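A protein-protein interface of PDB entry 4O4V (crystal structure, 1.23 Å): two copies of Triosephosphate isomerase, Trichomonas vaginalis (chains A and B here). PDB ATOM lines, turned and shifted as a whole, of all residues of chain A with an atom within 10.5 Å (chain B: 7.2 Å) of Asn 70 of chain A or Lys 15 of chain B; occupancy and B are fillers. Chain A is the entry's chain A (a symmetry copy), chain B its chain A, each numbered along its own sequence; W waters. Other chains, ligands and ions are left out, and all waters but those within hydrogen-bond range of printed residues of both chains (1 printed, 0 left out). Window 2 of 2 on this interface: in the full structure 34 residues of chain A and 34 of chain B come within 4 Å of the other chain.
O of Ala 12 of chain B is in hydrogen-bond range of N of Gly 71 of chain A (2.9 Å).
OD1 of Asn 13 of chain B lies within hydrogen-bond range of ND2 of Asn 70 of chain A (3.0 Å).
The backbone carbonyl oxygen (O) of Gly 71 of chain A is in hydrogen-bond range of the side-chain amide nitrogen (ND2) of Asn 13 of chain B (3.4 Å).
The backbone NH of Met 81 of chain A is in hydrogen-bond range of the backbone carbonyl oxygen of Lys 15 of chain B (3.1 Å).
N of Val 17 of chain B is in hydrogen-bond range of OG of Ser 84 of chain A.
O of Lys 15 of chain B sits close to O of Pro 80 of chain A.
The side-chain hydroxyl (OG1) of Thr 16 of chain B sits at hydrogen-bond distance from the side-chain carboxylate (OE1) of Glu 19 of chain B (2.8 Å).
O of Pro 69 of chain A lies within hydrogen-bond range of OG1 of Thr 78 of chain A.
The side-chain sulfur (SD) of Met 81 of chain A sits at hydrogen-bond distance from the backbone NH (N) of Thr 78 of chain A (3.6 Å).
The backbone carbonyl oxygen (O) of Met 81 of chain A is in hydrogen-bond range of the side-chain hydroxyl (OG) of Ser 84 of chain A, at 2.8 Å.
CG of Lys 15 of chain B touches O of Pro 69 of chain A (3.9 Å).
Asn 70 of chain A touches Ala 12 of chain B (CA to O, 3.1 Å).
Lys 15 of chain B touches Asn 70 of chain A.
O of Gly 71 of chain A touches CB of Lys 11 of chain B, at 3.5 Å.
Phe 73 of chain A touches Ala 12 of chain B.
Thr 74 of chain A touches Lys 11 of chain B (OG1 to CG, 3.4 Å).
CB of Ala 12 of chain B touches O of Glu 76 of chain A, 3.6 Å away.
CE of Met 81 of chain A touches O of Pro 14 of chain B, 3.6 Å away.
Phe 85 of chain A touches Val 17 of chain B (CZ to CG2, 3.6 Å).
Phe 85 of chain A touches Phe 46 of chain B (CE2 to CE1, 3.9 Å).
Lys 68 of chain A touches none of the printed residues of chain B.
Asn 70 of chain A touches just these residues of chain B: Ala 12, Asn 13 and Lys 15.
Printed residues of chain B within 4 Å of Glu 76 of chain A: Ala 12.
Of the printed residues of chain B, Phe 85 of chain A touches Val 17 and Phe 46.
Of the printed residues of chain A, Lys 11 of chain B touches Gly 71, Ala 72 and Thr 74.
Ala 12 of chain B touches five residues of chain A.
Of the printed residues of chain A, Lys 15 of chain B touches Pro 69, Asn 70, Pro 80 and Met 81.
Thr 16 of chain B touches one residue of chain A.
Printed residues of chain A within 4 Å of Phe 46 of chain B: Met 81 (3.7 Å) and Phe 85 (3.9 Å).
Leu 237 of chain B touches none of the printed residues of chain A.
The nearest residue of chain B that does not touch Asn 70 of chain A is Pro 14 of chain B (5.1 Å).
The nearest residue of chain A that does not touch Lys 15 of chain B is Ser 84 of chain A (4.4 Å).
The nearest printed residue of chain B that does not touch Thr 74 of chain A is Ala 12 of chain B (4.7 Å).
Water W1 lies within hydrogen-bond range of the side-chain amide nitrogen (ND2) of Asn 13 of chain B, the backbone NH (N) of Ala 72 of chain A and the backbone carbonyl oxygen (O) of Gly 71 of chain A.
Of the 12 printed residues of chain B, 9 touch a printed residue of chain A.
Printed residues of chain B that touch a printed residue of chain A: Lys 11, Ala 12, Asn 13, Pro 14, Lys 15, Thr 16, Val 17, Glu 18 and Phe 46.
Hydrophobic or aromatic side chains of chain B within 4 Å of the printed part of chain A: Ala 12, Val 17 and Phe 46.
Hydrophobic or aromatic side chains of chain A that line the printed part of chain B: Pro 80, Met 81 and Phe 85.
Among the printed residues, no Asp or Glu carboxylate lies within 4 Å of a Lys or Arg side-chain nitrogen of the other chain.
No position is printed for both chains.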
ATOM      1  N   VAL A  65      26.143 -24.695   1.318  1.00  0.00           N
ATOM      2  CA  VAL A  65      25.809 -25.483   0.122  1.00  0.00           C
ATOM      3  C   VAL A  65      24.488 -24.963  -0.404  1.00  0.00           C
ATOM      4  O   VAL A  65      23.724 -24.307   0.315  1.00  0.00           O
ATOM      5  CB  VAL A  65      25.666 -26.999   0.406  1.00  0.00           C
ATOM      6  CG1 VAL A  65      26.913 -27.599   0.952  1.00  0.00           C
ATOM      7  CG2 VAL A  65      24.518 -27.306   1.335  1.00  0.00           C
ATOM      8  N   PHE A  66      24.178 -25.250  -1.660  1.00  0.00           N
ATOM      9  CA  PHE A  66      22.876 -24.898  -2.216  1.00  0.00           C
ATOM     10  C   PHE A  66      21.837 -26.006  -1.931  1.00  0.00           C
ATOM     11  O   PHE A  66      22.130 -26.981  -1.273  1.00  0.00           O
ATOM     12  CB  PHE A  66      23.046 -24.582  -3.721  1.00  0.00           C
ATOM     13  CG  PHE A  66      21.856 -23.934  -4.351  1.00  0.00           C
ATOM     14  CD1 PHE A  66      21.351 -22.729  -3.901  1.00  0.00           C
ATOM     15  CD2 PHE A  66      21.218 -24.542  -5.432  1.00  0.00           C
ATOM     16  CE1 PHE A  66      20.260 -22.153  -4.494  1.00  0.00           C
ATOM     17  CE2 PHE A  66      20.128 -23.963  -6.010  1.00  0.00           C
ATOM     18  CZ  PHE A  66      19.640 -22.793  -5.556  1.00  0.00           C
ATOM     19  N   THR A  67      20.600 -25.817  -2.391  1.00  0.00           N
ATOM     20  CA  THR A  67      19.474 -26.714  -2.095  1.00  0.00           C
ATOM     21  C   THR A  67      19.245 -27.820  -3.119  1.00  0.00           C
ATOM     22  O   THR A  67      18.393 -28.677  -2.908  1.00  0.00           O
ATOM     23  CB  THR A  67      18.192 -25.909  -2.058  1.00  0.00           C
ATOM     24  OG1 THR A  67      18.163 -25.119  -3.243  1.00  0.00           O
ATOM     25  CG2 THR A  67      18.096 -25.023  -0.806  1.00  0.00           C
ATOM     26  N   LYS A  68      19.965 -27.799  -4.226  1.00  0.00           N
ATOM     27  CA  LYS A  68      19.739 -28.706  -5.346  1.00  0.00           C
ATOM     28  C   LYS A  68      21.020 -29.445  -5.712  1.00  0.00           C
ATOM     29  O   LYS A  68      22.106 -28.960  -5.390  1.00  0.00           O
ATOM     30  CB  LYS A  68      19.271 -27.880  -6.556  1.00  0.00           C
ATOM     31  CG  LYS A  68      17.997 -27.069  -6.321  1.00  0.00           C
ATOM     32  CD  LYS A  68      16.759 -27.921  -6.148  1.00  0.00           C
ATOM     33  CE  LYS A  68      15.518 -27.032  -6.067  1.00  0.00           C
ATOM     34  NZ  LYS A  68      14.262 -27.806  -5.925  1.00  0.00           N
ATOM     35  N   PRO A  69      20.934 -30.561  -6.451  1.00  0.00           N
ATOM     36  CA  PRO A  69      22.157 -31.316  -6.791  1.00  0.00           C
ATOM     37  C   PRO A  69      23.067 -30.649  -7.810  1.00  0.00           C
ATOM     38  O   PRO A  69      24.275 -30.872  -7.797  1.00  0.00           O
ATOM     39  CB  PRO A  69      21.626 -32.643  -7.344  1.00  0.00           C
ATOM     40  CG  PRO A  69      20.259 -32.317  -7.788  1.00  0.00           C
ATOM     41  CD  PRO A  69      19.718 -31.292  -6.825  1.00  0.00           C
ATOM     42  N   ASN A  70      22.477 -29.853  -8.701  1.00  0.00           N
ATOM     43  CA  ASN A  70      23.131 -29.258  -9.856  1.00  0.00           C
ATOM     44  C   ASN A  70      22.087 -28.486 -10.595  1.00  0.00           C
ATOM     45  O   ASN A  70      20.889 -28.636 -10.310  1.00  0.00           O
ATOM     46  CB  ASN A  70      23.767 -30.314 -10.802  1.00  0.00           C
ATOM     47  CG  ASN A  70      22.778 -31.193 -11.475  1.00  0.00           C
ATOM     48  OD1 ASN A  70      22.091 -31.965 -10.830  1.00  0.00           O
ATOM     49  ND2 ASN A  70      22.716 -31.114 -12.785  1.00  0.00           N
ATOM     50  N   GLY A  71      22.494 -27.692 -11.561  1.00  0.00           N
ATOM     51  CA  GLY A  71      21.584 -27.051 -12.491  1.00  0.00           C
ATOM     52  C   GLY A  71      21.868 -25.601 -12.724  1.00  0.00           C
ATOM     53  O   GLY A  71      23.007 -25.139 -12.602  1.00  0.00           O
ATOM     54  N   ALA A  72      20.817 -24.862 -13.055  1.00  0.00           N
ATOM     55  CA  ALA A  72      20.919 -23.492 -13.555  1.00  0.00           C
ATOM     56  C   ALA A  72      20.960 -22.507 -12.388  1.00  0.00           C
ATOM     57  O   ALA A  72      20.042 -21.697 -12.161  1.00  0.00           O
ATOM     58  CB  ALA A  72      19.766 -23.209 -14.495  1.00  0.00           C
ATOM     59  N   PHE A  73      22.064 -22.607 -11.654  1.00  0.00           N
ATOM     60  CA  PHE A  73      22.287 -21.846 -10.414  1.00  0.00           C
ATOM     61  C   PHE A  73      23.697 -21.268 -10.430  1.00  0.00           C
ATOM     62  O   PHE A  73      24.541 -21.631  -9.630  1.00  0.00           O
ATOM     63  CB  PHE A  73      22.034 -22.731  -9.200  1.00  0.00           C
ATOM     64  CG  PHE A  73      20.702 -23.459  -9.271  1.00  0.00           C
ATOM     65  CD1 PHE A  73      19.513 -22.762  -9.228  1.00  0.00           C
ATOM     66  CD2 PHE A  73      20.652 -24.840  -9.453  1.00  0.00           C
ATOM     67  CE1 PHE A  73      18.288 -23.436  -9.343  1.00  0.00           C
ATOM     68  CE2 PHE A  73      19.422 -25.500  -9.554  1.00  0.00           C
ATOM     69  CZ  PHE A  73      18.274 -24.790  -9.511  1.00  0.00           C
ATOM     70  N   THR A  74      23.933 -20.368 -11.372  1.00  0.00           N
ATOM     71  CA  THR A  74      25.247 -19.789 -11.554  1.00  0.00           C
ATOM     72  C   THR A  74      25.805 -19.269 -10.244  1.00  0.00           C
ATOM     73  O   THR A  74      25.120 -18.552  -9.511  1.00  0.00           O
ATOM     74  CB  THR A  74      25.173 -18.672 -12.619  1.00  0.00           C
ATOM     75  OG1 THR A  74      24.833 -19.262 -13.885  1.00  0.00           O
ATOM     76  CG2 THR A  74      26.497 -17.932 -12.793  1.00  0.00           C
ATOM     77  N   GLY A  75      27.039 -19.652  -9.939  1.00  0.00           N
ATOM     78  CA  GLY A  75      27.732 -19.232  -8.730  1.00  0.00           C
ATOM     79  C   GLY A  75      27.598 -20.166  -7.546  1.00  0.00           C
ATOM     80  O   GLY A  75      28.380 -20.032  -6.599  1.00  0.00           O
ATOM     81  N   GLU A  76      26.636 -21.088  -7.569  1.00  0.00           N
ATOM     82  CA  GLU A  76      26.396 -21.977  -6.428  1.00  0.00           C
ATOM     83  C   GLU A  76      27.224 -23.260  -6.513  1.00  0.00           C
ATOM     84  O   GLU A  76      27.454 -23.799  -7.580  1.00  0.00           O
ATOM     85  CB  GLU A  76      24.911 -22.325  -6.327  1.00  0.00           C
ATOM     86  CG  GLU A  76      24.022 -21.143  -6.008  1.00  0.00           C
ATOM     87  CD  GLU A  76      24.383 -20.472  -4.677  1.00  0.00           C
ATOM     88  OE1 GLU A  76      24.358 -21.151  -3.616  1.00  0.00           O
ATOM     89  OE2 GLU A  76      24.696 -19.253  -4.677  1.00  0.00           O
ATOM     90  N   VAL A  77      27.613 -23.768  -5.349  1.00  0.00           N
ATOM     91  CA  VAL A  77      28.270 -25.070  -5.199  1.00  0.00           C
ATOM     92  C   VAL A  77      27.316 -26.006  -4.496  1.00  0.00           C
ATOM     93  O   VAL A  77      26.590 -25.605  -3.589  1.00  0.00           O
ATOM     94  CB  VAL A  77      29.600 -24.924  -4.420  1.00  0.00           C
ATOM     95  CG1 VAL A  77      30.220 -26.274  -4.100  1.00  0.00           C
ATOM     96  CG2 VAL A  77      30.568 -24.067  -5.241  1.00  0.00           C
ATOM     97  N   THR A  78      27.263 -27.253  -4.954  1.00  0.00           N
ATOM     98  CA  THR A  78      26.249 -28.197  -4.493  1.00  0.00           C
ATOM     99  C   THR A  78      26.861 -29.376  -3.741  1.00  0.00           C
ATOM    100  O   THR A  78      28.065 -29.684  -3.821  1.00  0.00           O
ATOM    101  CB  THR A  78      25.434 -28.699  -5.661  1.00  0.00           C
ATOM    102  OG1 THR A  78      26.286 -29.513  -6.483  1.00  0.00           O
ATOM    103  CG2 THR A  78      24.831 -27.560  -6.468  1.00  0.00           C
ATOM    104  N   VAL A  79      25.999 -30.063  -2.997  1.00  0.00           N
ATOM    105  CA  VAL A  79      26.383 -31.223  -2.197  1.00  0.00           C
ATOM    106  C   VAL A  79      27.152 -32.281  -2.986  1.00  0.00           C
ATOM    107  O   VAL A  79      28.227 -32.698  -2.548  1.00  0.00           O
ATOM    108  CB  VAL A  79      25.178 -31.801  -1.454  1.00  0.00           C
ATOM    109  CG1 VAL A  79      25.493 -33.179  -0.858  1.00  0.00           C
ATOM    110  CG2 VAL A  79      24.715 -30.833  -0.352  1.00  0.00           C
ATOM    111  N   PRO A  80      26.653 -32.721  -4.155  1.00  0.00           N
ATOM    112  CA  PRO A  80      27.429 -33.761  -4.862  1.00  0.00           C
ATOM    113  C   PRO A  80      28.848 -33.311  -5.226  1.00  0.00           C
ATOM    114  O   PRO A  80      29.760 -34.126  -5.260  1.00  0.00           O
ATOM    115  CB  PRO A  80      26.591 -34.034  -6.117  1.00  0.00           C
ATOM    116  CG  PRO A  80      25.176 -33.563  -5.754  1.00  0.00           C
ATOM    117  CD  PRO A  80      25.347 -32.466  -4.795  1.00  0.00           C
ATOM    118  N   MET A  81      29.032 -32.028  -5.530  1.00  0.00           N
ATOM    119  CA  MET A  81      30.358 -31.548  -5.925  1.00  0.00           C
ATOM    120  C   MET A  81      31.319 -31.702  -4.751  1.00  0.00           C
ATOM    121  O   MET A  81      32.450 -32.165  -4.903  1.00  0.00           O
ATOM    122  CB  MET A  81      30.302 -30.093  -6.343  1.00  0.00           C
ATOM    123  CG  MET A  81      29.412 -29.765  -7.520  1.00  0.00           C
ATOM    124  SD  MET A  81      29.348 -27.976  -7.745  1.00  0.00           S
ATOM    125  CE  MET A  81      28.062 -27.858  -9.004  1.00  0.00           C
ATOM    126  N   ILE A  82      30.880 -31.275  -3.580  1.00  0.00           N
ATOM    127  CA  ILE A  82      31.665 -31.354  -2.359  1.00  0.00           C
ATOM    128  C   ILE A  82      31.940 -32.811  -2.007  1.00  0.00           C
ATOM    129  O   ILE A  82      33.079 -33.184  -1.702  1.00  0.00           O
ATOM    130  CB  ILE A  82      30.926 -30.603  -1.241  1.00  0.00           C
ATOM    131  CG1 ILE A  82      30.868 -29.094  -1.553  1.00  0.00           C
ATOM    132  CG2 ILE A  82      31.554 -30.856   0.121  1.00  0.00           C
ATOM    133  CD1 ILE A  82      29.730 -28.404  -0.824  1.00  0.00           C
ATOM    134  N   LYS A  83      30.920 -33.646  -2.065  1.00  0.00           N
ATOM    135  CA  LYS A  83      31.080 -35.058  -1.748  1.00  0.00           C
ATOM    136  C   LYS A  83      32.042 -35.735  -2.710  1.00  0.00           C
ATOM    137  O   LYS A  83      32.695 -36.721  -2.332  1.00  0.00           O
ATOM    138  CB  LYS A  83      29.742 -35.775  -1.766  1.00  0.00           C
ATOM    139  CG  LYS A  83      28.808 -35.391  -0.647  1.00  0.00           C
ATOM    140  CD  LYS A  83      27.592 -36.283  -0.657  1.00  0.00           C
ATOM    141  CE  LYS A  83      27.929 -37.699  -0.134  1.00  0.00           C
ATOM    142  NZ  LYS A  83      28.373 -37.742   1.283  1.00  0.00           N
ATOM    143  N   SER A  84      32.170 -35.250  -3.938  1.00  0.00           N
ATOM    144  CA  SER A  84      33.028 -35.913  -4.909  1.00  0.00           C
ATOM    145  C   SER A  84      34.501 -35.774  -4.554  1.00  0.00           C
ATOM    146  O   SER A  84      35.331 -36.527  -5.083  1.00  0.00           O
ATOM    147  CB  SER A  84      32.742 -35.407  -6.335  1.00  0.00           C
ATOM    148  OG  SER A  84      33.340 -34.142  -6.642  1.00  0.00           O
ATOM    149  N   PHE A  85      34.852 -34.855  -3.665  1.00  0.00           N
ATOM    150  CA  PHE A  85      36.199 -34.755  -3.113  1.00  0.00           C
ATOM    151  C   PHE A  85      36.360 -35.562  -1.828  1.00  0.00           C
ATOM    152  O   PHE A  85      37.459 -35.620  -1.296  1.00  0.00           O
ATOM    153  CB  PHE A  85      36.576 -33.290  -2.851  1.00  0.00           C
ATOM    154  CG  PHE A  85      36.786 -32.500  -4.101  1.00  0.00           C
ATOM    155  CD1 PHE A  85      38.027 -32.434  -4.696  1.00  0.00           C
ATOM    156  CD2 PHE A  85      35.732 -31.855  -4.720  1.00  0.00           C
ATOM    157  CE1 PHE A  85      38.213 -31.707  -5.874  1.00  0.00           C
ATOM    158  CE2 PHE A  85      35.913 -31.134  -5.874  1.00  0.00           C
ATOM    159  CZ  PHE A  85      37.145 -31.060  -6.456  1.00  0.00           C
ATOM    160  N   GLY A  86      35.294 -36.190  -1.334  1.00  0.00           N
ATOM    161  CA  GLY A  86      35.355 -36.916  -0.069  1.00  0.00           C
ATOM    162  C   GLY A  86      35.025 -36.088   1.149  1.00  0.00           C
ATOM    163  O   GLY A  86      35.229 -36.544   2.288  1.00  0.00           O
ATOM    164  N   ILE A  87      34.479 -34.898   0.954  1.00  0.00           N
ATOM    165  CA  ILE A  87      34.137 -33.970   2.047  1.00  0.00           C
ATOM    166  C   ILE A  87      32.738 -34.264   2.533  1.00  0.00           C
ATOM    167  O   ILE A  87      31.830 -34.417   1.727  1.00  0.00           O
ATOM    168  CB  ILE A  87      34.263 -32.526   1.552  1.00  0.00           C
ATOM    169  CG1 ILE A  87      35.716 -32.237   1.163  1.00  0.00           C
ATOM    170  CG2 ILE A  87      33.750 -31.554   2.606  1.00  0.00           C
ATOM    171  CD1 ILE A  87      35.898 -30.994   0.349  1.00  0.00           C
ATOM    172  N   PHE A 114      18.185 -31.418   2.331  1.00  0.00           N
ATOM    173  CA  PHE A 114      18.881 -31.896   1.143  1.00  0.00           C
ATOM    174  C   PHE A 114      20.269 -32.413   1.491  1.00  0.00           C
ATOM    175  O   PHE A 114      20.666 -33.488   1.033  1.00  0.00           O
ATOM    176  CB  PHE A 114      18.958 -30.801   0.083  1.00  0.00           C
ATOM    177  CG  PHE A 114      19.576 -31.268  -1.185  1.00  0.00           C
ATOM    178  CD1 PHE A 114      18.873 -32.055  -2.037  1.00  0.00           C
ATOM    179  CD2 PHE A 114      20.892 -30.929  -1.509  1.00  0.00           C
ATOM    180  CE1 PHE A 114      19.452 -32.533  -3.198  1.00  0.00           C
ATOM    181  CE2 PHE A 114      21.452 -31.395  -2.667  1.00  0.00           C
ATOM    182  CZ  PHE A 114      20.738 -32.194  -3.494  1.00  0.00           C
ATOM    183  N   ASN A 118      21.379 -36.555   1.450  1.00  0.00           N
ATOM    184  CA  ASN A 118      22.453 -36.901   0.517  1.00  0.00           C
ATOM    185  C   ASN A 118      23.770 -37.242   1.210  1.00  0.00           C
ATOM    186  O   ASN A 118      24.824 -37.228   0.591  1.00  0.00           O
ATOM    187  CB  ASN A 118      22.643 -35.778  -0.511  1.00  0.00           C
ATOM    188  CG  ASN A 118      21.564 -35.779  -1.556  1.00  0.00           C
ATOM    189  OD1 ASN A 118      21.712 -36.457  -2.585  1.00  0.00           O
ATOM    190  ND2 ASN A 118      20.464 -35.092  -1.320  1.00  0.00           N
ATOM    191  N   LYS B  11      27.553 -23.204 -15.104  1.00  0.00           N
ATOM    192  CA  LYS B  11      26.575 -23.000 -14.038  1.00  0.00           C
ATOM    193  C   LYS B  11      26.915 -23.952 -12.903  1.00  0.00           C
ATOM    194  O   LYS B  11      28.096 -24.187 -12.628  1.00  0.00           O
ATOM    195  CB  LYS B  11      25.121 -23.083 -14.511  1.00  0.00           C
ATOM    196  CG  LYS B  11      24.843 -22.175 -15.728  1.00  0.00           C
ATOM    197  CD  LYS B  11      23.387 -22.151 -16.109  1.00  0.00           C
ATOM    198  CE  LYS B  11      23.142 -21.244 -17.295  1.00  0.00           C
ATOM    199  NZ  LYS B  11      21.686 -21.115 -17.540  1.00  0.00           N
ATOM    200  N   ALA B  12      25.939 -24.497 -12.198  1.00  0.00           N
ATOM    201  CA  ALA B  12      26.195 -25.415 -11.077  1.00  0.00           C
ATOM    202  C   ALA B  12      26.255 -26.848 -11.595  1.00  0.00           C
ATOM    203  O   ALA B  12      25.395 -27.678 -11.304  1.00  0.00           O
ATOM    204  CB  ALA B  12      25.163 -25.255  -9.980  1.00  0.00           C
ATOM    205  N   ASN B  13      27.281 -27.100 -12.384  1.00  0.00           N
ATOM    206  CA  ASN B  13      27.474 -28.396 -13.034  1.00  0.00           C
ATOM    207  C   ASN B  13      28.955 -28.568 -13.306  1.00  0.00           C
ATOM    208  O   ASN B  13      29.702 -27.585 -13.343  1.00  0.00           O
ATOM    209  CB  ASN B  13      26.794 -28.447 -14.409  1.00  0.00           C
ATOM    210  CG  ASN B  13      25.315 -28.243 -14.379  1.00  0.00           C
ATOM    211  OD1 ASN B  13      24.551 -29.189 -14.109  1.00  0.00           O
ATOM    212  ND2 ASN B  13      24.868 -27.037 -14.670  1.00  0.00           N
ATOM    213  N   PRO B  14      29.405 -29.797 -13.558  1.00  0.00           N
ATOM    214  CA  PRO B  14      28.688 -31.056 -13.344  1.00  0.00           C
ATOM    215  C   PRO B  14      28.650 -31.401 -11.854  1.00  0.00           C
ATOM    216  O   PRO B  14      29.072 -30.617 -11.009  1.00  0.00           O
ATOM    217  CB  PRO B  14      29.534 -32.050 -14.166  1.00  0.00           C
ATOM    218  CG  PRO B  14      30.924 -31.534 -14.000  1.00  0.00           C
ATOM    219  CD  PRO B  14      30.786 -30.021 -14.011  1.00  0.00           C
ATOM    220  N   LYS B  15      28.117 -32.571 -11.524  1.00  0.00           N
ATOM    221  CA  LYS B  15      27.965 -32.971 -10.139  1.00  0.00           C
ATOM    222  C   LYS B  15      29.254 -33.393  -9.502  1.00  0.00           C
ATOM    223  O   LYS B  15      29.354 -33.341  -8.279  1.00  0.00           O
ATOM    224  CB  LYS B  15      26.969 -34.141 -10.028  1.00  0.00           C
ATOM    225  CG  LYS B  15      25.541 -33.702 -10.210  1.00  0.00           C
ATOM    226  CD  LYS B  15      24.498 -34.773  -9.868  1.00  0.00           C
ATOM    227  CE  LYS B  15      24.618 -35.972 -10.720  1.00  0.00           C
ATOM    228  NZ  LYS B  15      24.372 -35.620 -12.137  1.00  0.00           N
ATOM    229  N   THR B  16      30.243 -33.858 -10.273  1.00  0.00           N
ATOM    230  CA  THR B  16      31.433 -34.471  -9.684  1.00  0.00           C
ATOM    231  C   THR B  16      32.718 -33.990 -10.358  1.00  0.00           C
ATOM    232  O   THR B  16      32.744 -33.669 -11.554  1.00  0.00           O
ATOM    233  CB  THR B  16      31.415 -36.007  -9.763  1.00  0.00           C
ATOM    234  OG1 THR B  16      31.557 -36.415 -11.129  1.00  0.00           O
ATOM    235  CG2 THR B  16      30.134 -36.581  -9.161  1.00  0.00           C
ATOM    236  N   VAL B  17      33.802 -34.011  -9.592  1.00  0.00           N
ATOM    237  CA  VAL B  17      35.099 -33.645 -10.131  1.00  0.00           C
ATOM    238  C   VAL B  17      35.518 -34.594 -11.270  1.00  0.00           C
ATOM    239  O   VAL B  17      36.152 -34.147 -12.228  1.00  0.00           O
ATOM    240  CB  VAL B  17      36.174 -33.544  -9.023  1.00  0.00           C
ATOM    241  CG1 VAL B  17      36.451 -34.906  -8.369  1.00  0.00           C
ATOM    242  CG2 VAL B  17      37.431 -32.899  -9.585  1.00  0.00           C
ATOM    243  N   GLU B  18      35.160 -35.872 -11.210  1.00  0.00           N
ATOM    244  CA  GLU B  18      35.492 -36.787 -12.300  1.00  0.00           C
ATOM    245  C   GLU B  18      34.823 -36.346 -13.604  1.00  0.00           C
ATOM    246  O   GLU B  18      35.438 -36.385 -14.665  1.00  0.00           O
ATOM    247  CB  GLU B  18      35.096 -38.211 -11.906  1.00  0.00           C
ATOM    248  CG  GLU B  18      35.917 -38.767 -10.767  1.00  0.00           C
ATOM    249  CD  GLU B  18      35.350 -38.487  -9.341  1.00  0.00           C
ATOM    250  OE1 GLU B  18      34.392 -37.679  -9.088  1.00  0.00           O
ATOM    251  OE2 GLU B  18      35.908 -39.118  -8.410  1.00  0.00           O
ATOM    252  N   GLU B  19      33.558 -35.925 -13.521  1.00  0.00           N
ATOM    253  CA  GLU B  19      32.876 -35.422 -14.703  1.00  0.00           C
ATOM    254  C   GLU B  19      33.515 -34.131 -15.221  1.00  0.00           C
ATOM    255  O   GLU B  19      33.614 -33.919 -16.435  1.00  0.00           O
ATOM    256  CB  GLU B  19      31.410 -35.195 -14.408  1.00  0.00           C
ATOM    257  CG  GLU B  19      30.567 -36.433 -14.276  1.00  0.00           C
ATOM    258  CD  GLU B  19      29.212 -36.063 -13.703  1.00  0.00           C
ATOM    259  OE1 GLU B  19      29.116 -35.866 -12.485  1.00  0.00           O
ATOM    260  OE2 GLU B  19      28.257 -35.868 -14.481  1.00  0.00           O
ATOM    261  N   ALA B  20      33.956 -33.273 -14.301  1.00  0.00           N
ATOM    262  CA  ALA B  20      34.636 -32.042 -14.718  1.00  0.00           C
ATOM    263  C   ALA B  20      35.905 -32.388 -15.476  1.00  0.00           C
ATOM    264  O   ALA B  20      36.214 -31.776 -16.495  1.00  0.00           O
ATOM    265  CB  ALA B  20      34.942 -31.192 -13.521  1.00  0.00           C
ATOM    266  N   PHE B  46      35.630 -26.547  -8.426  1.00  0.00           N
ATOM    267  CA  PHE B  46      36.299 -27.124  -9.589  1.00  0.00           C
ATOM    268  C   PHE B  46      37.311 -26.180 -10.237  1.00  0.00           C
ATOM    269  O   PHE B  46      38.040 -26.590 -11.145  1.00  0.00           O
ATOM    270  CB  PHE B  46      35.285 -27.541 -10.665  1.00  0.00           C
ATOM    271  CG  PHE B  46      34.310 -28.613 -10.246  1.00  0.00           C
ATOM    272  CD1 PHE B  46      34.635 -29.613  -9.339  1.00  0.00           C
ATOM    273  CD2 PHE B  46      33.034 -28.626 -10.782  1.00  0.00           C
ATOM    274  CE1 PHE B  46      33.677 -30.589  -8.971  1.00  0.00           C
ATOM    275  CE2 PHE B  46      32.088 -29.598 -10.415  1.00  0.00           C
ATOM    276  CZ  PHE B  46      32.427 -30.586  -9.529  1.00  0.00           C
ATOM    277  N   LEU B 237      28.556 -27.771 -21.647  1.00  0.00           N
ATOM    278  CA  LEU B 237      28.843 -29.060 -21.045  1.00  0.00           C
ATOM    279  C   LEU B 237      28.879 -30.160 -22.100  1.00  0.00           C
ATOM    280  O   LEU B 237      29.018 -31.331 -21.762  1.00  0.00           O
ATOM    281  CB  LEU B 237      27.740 -29.399 -20.023  1.00  0.00           C
ATOM    282  CG  LEU B 237      27.558 -28.374 -18.898  1.00  0.00           C
ATOM    283  CD1 LEU B 237      26.337 -28.696 -18.056  1.00  0.00           C
ATOM    284  CD2 LEU B 237      28.791 -28.328 -18.019  1.00  0.00           C
HETATM  285  O   HOH W   1      22.159 -26.196 -15.596  1.00  0.00           O
